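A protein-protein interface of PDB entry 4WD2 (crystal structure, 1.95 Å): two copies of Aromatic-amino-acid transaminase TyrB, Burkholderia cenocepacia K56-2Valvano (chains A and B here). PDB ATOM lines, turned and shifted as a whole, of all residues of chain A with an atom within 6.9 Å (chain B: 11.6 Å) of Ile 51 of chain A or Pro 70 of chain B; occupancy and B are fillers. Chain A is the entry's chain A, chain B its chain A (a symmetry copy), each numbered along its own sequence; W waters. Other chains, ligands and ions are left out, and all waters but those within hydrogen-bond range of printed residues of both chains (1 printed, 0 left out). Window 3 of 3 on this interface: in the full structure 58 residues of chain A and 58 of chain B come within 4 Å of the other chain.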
ATOM      1  N   ILE A  41       0.700 -10.011  27.191  1.00  0.00           N
ATOM      2  CA  ILE A  41       1.081  -9.200  26.033  1.00  0.00           C
ATOM      3  C   ILE A  41       0.666  -9.885  24.725  1.00  0.00           C
ATOM      4  O   ILE A  41       1.139 -10.976  24.392  1.00  0.00           O
ATOM      5  CB  ILE A  41       2.592  -8.907  26.030  1.00  0.00           C
ATOM      6  CG1 ILE A  41       2.981  -8.233  27.348  1.00  0.00           C
ATOM      7  CG2 ILE A  41       2.966  -8.013  24.848  1.00  0.00           C
ATOM      8  CD1 ILE A  41       4.471  -8.191  27.615  1.00  0.00           C
ATOM      9  N   ILE A  43       1.116 -10.190  21.479  1.00  0.00           N
ATOM     10  CA  ILE A  43       1.941 -10.172  20.275  1.00  0.00           C
ATOM     11  C   ILE A  43       2.615 -11.537  20.138  1.00  0.00           C
ATOM     12  O   ILE A  43       2.617 -12.311  21.087  1.00  0.00           O
ATOM     13  CB  ILE A  43       3.015  -9.062  20.319  1.00  0.00           C
ATOM     14  CG1 ILE A  43       3.998  -9.297  21.459  1.00  0.00           C
ATOM     15  CG2 ILE A  43       2.384  -7.678  20.454  1.00  0.00           C
ATOM     16  CD1 ILE A  43       5.072  -8.226  21.539  1.00  0.00           C
ATOM     17  N   TYR A  44       3.182 -11.837  18.972  1.00  0.00           N
ATOM     18  CA  TYR A  44       3.841 -13.129  18.787  1.00  0.00           C
ATOM     19  C   TYR A  44       5.254 -13.154  19.376  1.00  0.00           C
ATOM     20  O   TYR A  44       6.066 -12.270  19.111  1.00  0.00           O
ATOM     21  CB  TYR A  44       3.902 -13.520  17.305  1.00  0.00           C
ATOM     22  CG  TYR A  44       4.561 -14.873  17.088  1.00  0.00           C
ATOM     23  CD1 TYR A  44       3.827 -16.050  17.171  1.00  0.00           C
ATOM     24  CD2 TYR A  44       5.923 -14.973  16.820  1.00  0.00           C
ATOM     25  CE1 TYR A  44       4.431 -17.287  16.983  1.00  0.00           C
ATOM     26  CE2 TYR A  44       6.535 -16.205  16.639  1.00  0.00           C
ATOM     27  CZ  TYR A  44       5.787 -17.352  16.721  1.00  0.00           C
ATOM     28  OH  TYR A  44       6.400 -18.565  16.538  1.00  0.00           O
ATOM     29  N   PHE A  45       5.527 -14.177  20.182  1.00  0.00           N
ATOM     30  CA  PHE A  45       6.877 -14.485  20.645  1.00  0.00           C
ATOM     31  C   PHE A  45       7.287 -15.830  20.047  1.00  0.00           C
ATOM     32  O   PHE A  45       6.434 -16.662  19.768  1.00  0.00           O
ATOM     33  CB  PHE A  45       6.944 -14.525  22.174  1.00  0.00           C
ATOM     34  CG  PHE A  45       6.498 -13.252  22.826  1.00  0.00           C
ATOM     35  CD1 PHE A  45       5.157 -13.015  23.074  1.00  0.00           C
ATOM     36  CD2 PHE A  45       7.420 -12.282  23.180  1.00  0.00           C
ATOM     37  CE1 PHE A  45       4.741 -11.833  23.670  1.00  0.00           C
ATOM     38  CE2 PHE A  45       7.018 -11.095  23.777  1.00  0.00           C
ATOM     39  CZ  PHE A  45       5.678 -10.868  24.023  1.00  0.00           C
ATOM     40  N   ASP A  46       8.580 -16.046  19.837  1.00  0.00           N
ATOM     41  CA  ASP A  46       9.021 -17.299  19.235  1.00  0.00           C
ATOM     42  C   ASP A  46       9.282 -18.369  20.292  1.00  0.00           C
ATOM     43  O   ASP A  46       8.885 -18.223  21.449  1.00  0.00           O
ATOM     44  CB  ASP A  46      10.273 -17.084  18.363  1.00  0.00           C
ATOM     45  CG  ASP A  46      11.454 -16.475  19.125  1.00  0.00           C
ATOM     46  OD1 ASP A  46      11.514 -16.562  20.371  1.00  0.00           O
ATOM     47  OD2 ASP A  46      12.348 -15.915  18.454  1.00  0.00           O
ATOM     48  N   GLU A  48      11.821 -19.090  21.840  1.00  0.00           N
ATOM     49  CA  GLU A  48      12.700 -18.644  22.912  1.00  0.00           C
ATOM     50  C   GLU A  48      12.093 -17.472  23.684  1.00  0.00           C
ATOM     51  O   GLU A  48      12.762 -16.848  24.505  1.00  0.00           O
ATOM     52  CB  GLU A  48      14.076 -18.261  22.348  1.00  0.00           C
ATOM     53  N   GLY A  49      10.821 -17.181  23.423  1.00  0.00           N
ATOM     54  CA  GLY A  49      10.125 -16.104  24.108  1.00  0.00           C
ATOM     55  C   GLY A  49      10.559 -14.710  23.690  1.00  0.00           C
ATOM     56  O   GLY A  49      10.370 -13.744  24.437  1.00  0.00           O
ATOM     57  N   ARG A  50      11.139 -14.594  22.499  1.00  0.00           N
ATOM     58  CA  ARG A  50      11.543 -13.289  21.973  1.00  0.00           C
ATOM     59  C   ARG A  50      10.636 -12.834  20.836  1.00  0.00           C
ATOM     60  O   ARG A  50      10.046 -13.654  20.138  1.00  0.00           O
ATOM     61  CB  ARG A  50      12.983 -13.322  21.466  1.00  0.00           C
ATOM     62  CG  ARG A  50      13.990 -13.937  22.405  1.00  0.00           C
ATOM     63  CD  ARG A  50      15.386 -13.792  21.825  1.00  0.00           C
ATOM     64  NE  ARG A  50      16.411 -14.323  22.712  1.00  0.00           N
ATOM     65  CZ  ARG A  50      17.047 -15.475  22.514  1.00  0.00           C
ATOM     66  NH1 ARG A  50      16.765 -16.220  21.449  1.00  0.00           N
ATOM     67  NH2 ARG A  50      17.966 -15.882  23.378  1.00  0.00           N
ATOM     68  N   ILE A  51      10.529 -11.521  20.654  1.00  0.00           N
ATOM     69  CA  ILE A  51       9.901 -10.968  19.461  1.00  0.00           C
ATOM     70  C   ILE A  51      10.862 -11.138  18.294  1.00  0.00           C
ATOM     71  O   ILE A  51      11.957 -10.568  18.304  1.00  0.00           O
ATOM     72  CB  ILE A  51       9.558  -9.484  19.626  1.00  0.00           C
ATOM     73  CG1 ILE A  51       8.746  -9.258  20.903  1.00  0.00           C
ATOM     74  CG2 ILE A  51       8.829  -8.964  18.386  1.00  0.00           C
ATOM     75  CD1 ILE A  51       8.641  -7.795  21.309  1.00  0.00           C
ATOM     76  N   PRO A  52      10.462 -11.925  17.281  1.00  0.00           N
ATOM     77  CA  PRO A  52      11.425 -12.219  16.213  1.00  0.00           C
ATOM     78  C   PRO A  52      11.595 -11.093  15.200  1.00  0.00           C
ATOM     79  O   PRO A  52      10.724 -10.239  15.033  1.00  0.00           O
ATOM     80  CB  PRO A  52      10.830 -13.460  15.536  1.00  0.00           C
ATOM     81  CG  PRO A  52       9.357 -13.343  15.772  1.00  0.00           C
ATOM     82  CD  PRO A  52       9.203 -12.679  17.120  1.00  0.00           C
ATOM     83  N   VAL A  53      12.751 -11.097  14.551  1.00  0.00           N
ATOM     84  CA  VAL A  53      12.955 -10.367  13.308  1.00  0.00           C
ATOM     85  C   VAL A  53      12.956 -11.409  12.200  1.00  0.00           C
ATOM     86  O   VAL A  53      13.877 -12.226  12.128  1.00  0.00           O
ATOM     87  CB  VAL A  53      14.282  -9.584  13.299  1.00  0.00           C
ATOM     88  CG1 VAL A  53      14.573  -9.059  11.904  1.00  0.00           C
ATOM     89  CG2 VAL A  53      14.236  -8.446  14.299  1.00  0.00           C
ATOM     90  N   ARG A  58      14.713  -9.163   7.563  1.00  0.00           N
ATOM     91  CA  ARG A  58      16.114  -8.792   7.737  1.00  0.00           C
ATOM     92  C   ARG A  58      16.825  -8.715   6.387  1.00  0.00           C
ATOM     93  O   ARG A  58      17.541  -7.761   6.107  1.00  0.00           O
ATOM     94  CB  ARG A  58      16.820  -9.791   8.655  1.00  0.00           C
ATOM     95  CG  ARG A  58      18.307  -9.528   8.847  1.00  0.00           C
ATOM     96  CD  ARG A  58      18.941 -10.614   9.706  1.00  0.00           C
ATOM     97  NE  ARG A  58      18.319 -10.691  11.026  1.00  0.00           N
ATOM     98  CZ  ARG A  58      18.729  -9.993  12.080  1.00  0.00           C
ATOM     99  NH1 ARG A  58      19.769  -9.172  11.969  1.00  0.00           N
ATOM    100  NH2 ARG A  58      18.106 -10.120  13.244  1.00  0.00           N
ATOM    101  N   SER A 257       5.875  -9.207  11.865  1.00  0.00           N
ATOM    102  CA  SER A 257       6.540  -8.846  13.117  1.00  0.00           C
ATOM    103  C   SER A 257       7.043  -7.400  13.031  1.00  0.00           C
ATOM    104  O   SER A 257       8.111  -7.067  13.535  1.00  0.00           O
ATOM    105  CB  SER A 257       7.689  -9.817  13.418  1.00  0.00           C
ATOM    106  OG  SER A 257       8.066  -9.763  14.781  1.00  0.00           O
ATOM    107  N   TYR A 259       5.287  -4.573  14.091  1.00  0.00           N
ATOM    108  CA  TYR A 259       4.369  -3.777  14.904  1.00  0.00           C
ATOM    109  C   TYR A 259       4.717  -2.294  14.879  1.00  0.00           C
ATOM    110  O   TYR A 259       3.869  -1.457  14.589  1.00  0.00           O
ATOM    111  CB  TYR A 259       4.368  -4.264  16.357  1.00  0.00           C
ATOM    112  CG  TYR A 259       4.250  -5.759  16.505  1.00  0.00           C
ATOM    113  CD1 TYR A 259       3.007  -6.367  16.654  1.00  0.00           C
ATOM    114  CD2 TYR A 259       5.382  -6.565  16.495  1.00  0.00           C
ATOM    115  CE1 TYR A 259       2.898  -7.742  16.781  1.00  0.00           C
ATOM    116  CE2 TYR A 259       5.282  -7.938  16.616  1.00  0.00           C
ATOM    117  CZ  TYR A 259       4.041  -8.519  16.764  1.00  0.00           C
ATOM    118  OH  TYR A 259       3.947  -9.884  16.887  1.00  0.00           O
ATOM    119  N   LEU B  64      22.286   2.915  12.685  1.00  0.00           N
ATOM    120  CA  LEU B  64      21.078   2.187  13.065  1.00  0.00           C
ATOM    121  C   LEU B  64      21.002   0.822  12.386  1.00  0.00           C
ATOM    122  O   LEU B  64      20.413  -0.116  12.925  1.00  0.00           O
ATOM    123  CB  LEU B  64      19.833   3.009  12.725  1.00  0.00           C
ATOM    124  CG  LEU B  64      19.623   4.276  13.559  1.00  0.00           C
ATOM    125  CD1 LEU B  64      18.574   5.169  12.916  1.00  0.00           C
ATOM    126  CD2 LEU B  64      19.236   3.928  14.992  1.00  0.00           C
ATOM    127  N   GLN B  65      21.604   0.722  11.205  1.00  0.00           N
ATOM    128  CA  GLN B  65      21.587  -0.506  10.412  1.00  0.00           C
ATOM    129  C   GLN B  65      22.354  -1.623  11.098  1.00  0.00           C
ATOM    130  O   GLN B  65      21.994  -2.795  10.989  1.00  0.00           O
ATOM    131  CB  GLN B  65      22.174  -0.254   9.021  1.00  0.00           C
ATOM    132  N   ARG B  66      23.411  -1.252  11.811  1.00  0.00           N
ATOM    133  CA  ARG B  66      24.222  -2.218  12.540  1.00  0.00           C
ATOM    134  C   ARG B  66      23.519  -2.649  13.823  1.00  0.00           C
ATOM    135  O   ARG B  66      24.079  -3.388  14.629  1.00  0.00           O
ATOM    136  CB  ARG B  66      25.601  -1.633  12.854  1.00  0.00           C
ATOM    137  N   ASP B  67      22.292  -2.180  14.008  1.00  0.00           N
ATOM    138  CA  ASP B  67      21.484  -2.573  15.154  1.00  0.00           C
ATOM    139  C   ASP B  67      20.140  -3.155  14.703  1.00  0.00           C
ATOM    140  O   ASP B  67      19.123  -2.460  14.680  1.00  0.00           O
ATOM    141  CB  ASP B  67      21.262  -1.378  16.083  1.00  0.00           C
ATOM    142  N   SER B  68      20.145  -4.436  14.346  1.00  0.00           N
ATOM    143  CA  SER B  68      18.929  -5.106  13.901  1.00  0.00           C
ATOM    144  C   SER B  68      18.224  -5.826  15.051  1.00  0.00           C
ATOM    145  O   SER B  68      18.518  -6.988  15.348  1.00  0.00           O
ATOM    146  CB  SER B  68      19.246  -6.098  12.781  1.00  0.00           C
ATOM    147  N   GLY B  69      17.288  -5.129  15.692  1.00  0.00           N
ATOM    148  CA  GLY B  69      16.496  -5.711  16.760  1.00  0.00           C
ATOM    149  C   GLY B  69      15.017  -5.735  16.417  1.00  0.00           C
ATOM    150  O   GLY B  69      14.623  -5.248  15.354  1.00  0.00           O
ATOM    151  N   PRO B  70      14.190  -6.300  17.315  1.00  0.00           N
ATOM    152  CA  PRO B  70      12.742  -6.414  17.096  1.00  0.00           C
ATOM    153  C   PRO B  70      12.075  -5.053  17.053  1.00  0.00           C
ATOM    154  O   PRO B  70      12.665  -4.073  17.508  1.00  0.00           O
ATOM    155  CB  PRO B  70      12.260  -7.221  18.306  1.00  0.00           C
ATOM    156  CG  PRO B  70      13.289  -6.962  19.363  1.00  0.00           C
ATOM    157  CD  PRO B  70      14.593  -6.832  18.629  1.00  0.00           C
ATOM    158  N   LYS B  71      10.864  -4.985  16.510  1.00  0.00           N
ATOM    159  CA  LYS B  71      10.163  -3.713  16.398  1.00  0.00           C
ATOM    160  C   LYS B  71       8.809  -3.766  17.103  1.00  0.00           C
ATOM    161  O   LYS B  71       7.776  -3.920  16.457  1.00  0.00           O
ATOM    162  CB  LYS B  71       9.992  -3.328  14.925  1.00  0.00           C
ATOM    163  CG  LYS B  71      11.309  -3.063  14.199  1.00  0.00           C
ATOM    164  CD  LYS B  71      11.976  -1.785  14.715  1.00  0.00           C
ATOM    165  CE  LYS B  71      13.473  -1.753  14.409  1.00  0.00           C
ATOM    166  NZ  LYS B  71      14.111  -0.480  14.867  1.00  0.00           N
ATOM    167  N   PRO B  72       8.815  -3.644  18.441  1.00  0.00           N
ATOM    168  CA  PRO B  72       7.562  -3.622  19.197  1.00  0.00           C
ATOM    169  C   PRO B  72       6.812  -2.305  19.027  1.00  0.00           C
ATOM    170  O   PRO B  72       7.381  -1.329  18.526  1.00  0.00           O
ATOM    171  CB  PRO B  72       8.026  -3.797  20.646  1.00  0.00           C
ATOM    172  CG  PRO B  72       9.382  -3.170  20.658  1.00  0.00           C
ATOM    173  CD  PRO B  72       9.988  -3.541  19.327  1.00  0.00           C
ATOM    174  N   TYR B  73       5.546  -2.292  19.433  1.00  0.00           N
ATOM    175  CA  TYR B  73       4.764  -1.065  19.426  1.00  0.00           C
ATOM    176  C   TYR B  73       5.436  -0.013  20.290  1.00  0.00           C
ATOM    177  O   TYR B  73       5.894  -0.307  21.399  1.00  0.00           O
ATOM    178  CB  TYR B  73       3.337  -1.302  19.944  1.00  0.00           C
ATOM    179  CG  TYR B  73       2.440  -2.147  19.067  1.00  0.00           C
ATOM    180  CD1 TYR B  73       1.970  -1.666  17.855  1.00  0.00           C
ATOM    181  CD2 TYR B  73       2.024  -3.410  19.477  1.00  0.00           C
ATOM    182  CE1 TYR B  73       1.140  -2.423  17.060  1.00  0.00           C
ATOM    183  CE2 TYR B  73       1.184  -4.177  18.685  1.00  0.00           C
ATOM    184  CZ  TYR B  73       0.750  -3.676  17.479  1.00  0.00           C
ATOM    185  OH  TYR B  73      -0.078  -4.421  16.687  1.00  0.00           O
ATOM    186  N   LEU B  74       5.499   1.206  19.771  1.00  0.00           N
ATOM    187  CA  LEU B  74       5.890   2.368  20.555  1.00  0.00           C
ATOM    188  C   LEU B  74       4.703   2.793  21.412  1.00  0.00           C
ATOM    189  O   LEU B  74       3.577   2.368  21.148  1.00  0.00           O
ATOM    190  CB  LEU B  74       6.336   3.519  19.640  1.00  0.00           C
ATOM    191  CG  LEU B  74       7.576   3.350  18.749  1.00  0.00           C
ATOM    192  CD1 LEU B  74       7.860   4.635  17.980  1.00  0.00           C
ATOM    193  CD2 LEU B  74       8.790   2.949  19.571  1.00  0.00           C
ATOM    194  N   LEU B  79       8.289   7.663  20.727  1.00  0.00           N
ATOM    195  CA  LEU B  79       9.570   7.429  21.388  1.00  0.00           C
ATOM    196  C   LEU B  79       9.933   8.542  22.379  1.00  0.00           C
ATOM    197  O   LEU B  79       9.939   9.721  22.018  1.00  0.00           O
ATOM    198  CB  LEU B  79      10.664   7.286  20.326  1.00  0.00           C
ATOM    199  CG  LEU B  79      11.962   6.556  20.662  1.00  0.00           C
ATOM    200  CD1 LEU B  79      11.676   5.095  20.966  1.00  0.00           C
ATOM    201  CD2 LEU B  79      12.955   6.690  19.503  1.00  0.00           C
ATOM    202  N   PRO B 294       2.735   5.659  16.697  1.00  0.00           N
ATOM    203  CA  PRO B 294       3.503   6.083  15.518  1.00  0.00           C
ATOM    204  C   PRO B 294       4.634   5.125  15.155  1.00  0.00           C
ATOM    205  O   PRO B 294       4.888   4.186  15.908  1.00  0.00           O
ATOM    206  CB  PRO B 294       4.061   7.434  15.948  1.00  0.00           C
ATOM    207  CG  PRO B 294       4.311   7.241  17.416  1.00  0.00           C
ATOM    208  CD  PRO B 294       3.204   6.342  17.918  1.00  0.00           C
ATOM    209  N   GLN B 295       5.310   5.378  14.032  1.00  0.00           N
ATOM    210  CA  GLN B 295       6.307   4.451  13.505  1.00  0.00           C
ATOM    211  C   GLN B 295       7.707   4.716  14.048  1.00  0.00           C
ATOM    212  O   GLN B 295       8.001   5.780  14.601  1.00  0.00           O
ATOM    213  CB  GLN B 295       6.328   4.486  11.969  1.00  0.00           C
ATOM    214  CG  GLN B 295       7.129   5.627  11.341  1.00  0.00           C
ATOM    215  CD  GLN B 295       6.412   6.975  11.388  1.00  0.00           C
ATOM    216  OE1 GLN B 295       5.553   7.216  12.232  1.00  0.00           O
ATOM    217  NE2 GLN B 295       6.768   7.858  10.471  1.00  0.00           N
ATOM    218  N   THR B 296       8.570   3.726  13.867  1.00  0.00           N
ATOM    219  CA  THR B 296       9.835   3.671  14.581  1.00  0.00           C
ATOM    220  C   THR B 296      11.007   4.217  13.775  1.00  0.00           C
ATOM    221  O   THR B 296      11.836   4.954  14.296  1.00  0.00           O
ATOM    222  CB  THR B 296      10.142   2.219  15.001  1.00  0.00           C
ATOM    223  OG1 THR B 296       9.143   1.767  15.923  1.00  0.00           O
ATOM    224  CG2 THR B 296      11.509   2.110  15.651  1.00  0.00           C
ATOM    225  N   TYR B 297      11.074   3.852  12.502  1.00  0.00           N
ATOM    226  CA  TYR B 297      12.278   4.100  11.719  1.00  0.00           C
ATOM    227  C   TYR B 297      12.686   5.580  11.687  1.00  0.00           C
ATOM    228  O   TYR B 297      13.751   5.938  12.192  1.00  0.00           O
ATOM    229  CB  TYR B 297      12.104   3.581  10.295  1.00  0.00           C
ATOM    230  CG  TYR B 297      13.382   3.683   9.510  1.00  0.00           C
ATOM    231  CD1 TYR B 297      13.549   4.662   8.546  1.00  0.00           C
ATOM    232  CD2 TYR B 297      14.441   2.819   9.765  1.00  0.00           C
ATOM    233  CE1 TYR B 297      14.726   4.770   7.837  1.00  0.00           C
ATOM    234  CE2 TYR B 297      15.629   2.921   9.063  1.00  0.00           C
ATOM    235  CZ  TYR B 297      15.763   3.896   8.096  1.00  0.00           C
ATOM    236  OH  TYR B 297      16.945   4.004   7.388  1.00  0.00           O
ATOM    237  N   LYS B 300      13.683   7.115  15.094  1.00  0.00           N
ATOM    238  CA  LYS B 300      15.007   6.668  15.519  1.00  0.00           C
ATOM    239  C   LYS B 300      16.098   7.478  14.837  1.00  0.00           C
ATOM    240  O   LYS B 300      17.077   7.854  15.473  1.00  0.00           O
ATOM    241  CB  LYS B 300      15.211   5.179  15.221  1.00  0.00           C
ATOM    242  CG  LYS B 300      14.497   4.226  16.170  1.00  0.00           C
ATOM    243  CD  LYS B 300      15.074   4.260  17.584  1.00  0.00           C
ATOM    244  CE  LYS B 300      14.688   3.005  18.359  1.00  0.00           C
ATOM    245  NZ  LYS B 300      14.978   3.108  19.824  1.00  0.00           N
HETATM  246  O   HOH W   1      10.484  -7.224  14.953  1.00  0.00           O
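Printed residues of chain A that touch a printed residue of chain B: Ile 51, Val 53, Arg 58 and Tyr 259.
Hydrophobic or aromatic side chains of chain A that line the printed part of chain B: Ile 51, Val 53 and Tyr 259.
Hydrophobic or aromatic side chains of chain B that line the printed part of chain A: Pro 70 and Tyr 73.
Among the printed residues, no Asp or Glu carboxylate lies within 4 Å of a Lys or Arg side-chain nitrogen of the other chain.
Ile 51 of chain A touches Pro 70 of chain B (O to CB, 3.4 Å).
CG2 of Val 53 of chain A touches O of Gly 69 of chain B, at 3.4 Å.
Val 53 of chain A touches Pro 70 of chain B.
Arg 58 of chain A touches Ser 68 of chain B.
Tyr 259 of chain A touches Tyr 73 of chain B (CD1 to CE2, 3.5 Å).
OH of Tyr 259 of chain A lies within hydrogen-bond range of N of Tyr 44 of chain A (3.0 Å).
Water W1 lies within hydrogen-bond range of the backbone NH (N) of Lys 71 of chain B (2.8 Å), the backbone carbonyl oxygen (O) of Ser 257 of chain A (2.8 Å) and the backbone carbonyl oxygen (O) of Pro 52 of chain A (3.0 Å).
N of Tyr 259 of chain A sits close to O of Lys 71 of chain B (3.5 Å).
No position is printed for both chains.
Of the 6 pairs that touch across the chains among the printed residues, none has its exchanged pair printed and touching as well.
Of chain B, only Pro 70 (3.4 Å) comes within 4 Å of Ile 51 of chain A.
Pro 70 of chain B touches two residues of chain A.
No residue of chain B comes within 4 Å of Phe 45 of chain A.
No residue of chain B comes within 4 Å of Gly 49 of chain A.
No residue of chain B comes within 4 Å of Pro 52 of chain A.
Printed residues of chain B within 4 Å of Val 53 of chain A: Gly 69 (3.4 Å) and Pro 70 (3.7 Å).
No residue of chain B comes within 4 Å of Ser 257 of chain A.
Of the printed residues of chain B, Tyr 259 of chain A touches Lys 71 and Tyr 73.
Printed residues of chain A within 4 Å of Lys 71 of chain B: Tyr 259 (3.4 Å).
Printed residues of chain A within 4 Å of Gly 69 of chain B: Val 53.
Printed residues of chain B within 4 Å of Arg 58 of chain A: Ser 68.
The nearest residue of chain B that does not touch Ile 51 of chain A is Pro 72 of chain B (4.1 Å).
The nearest residue of chain A that does not touch Pro 70 of chain B is Pro 52 of chain A (4.7 Å).
The nearest printed residue of chain A that does not touch Lys 71 of chain B is Ser 257 of chain A (4.3 Å).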
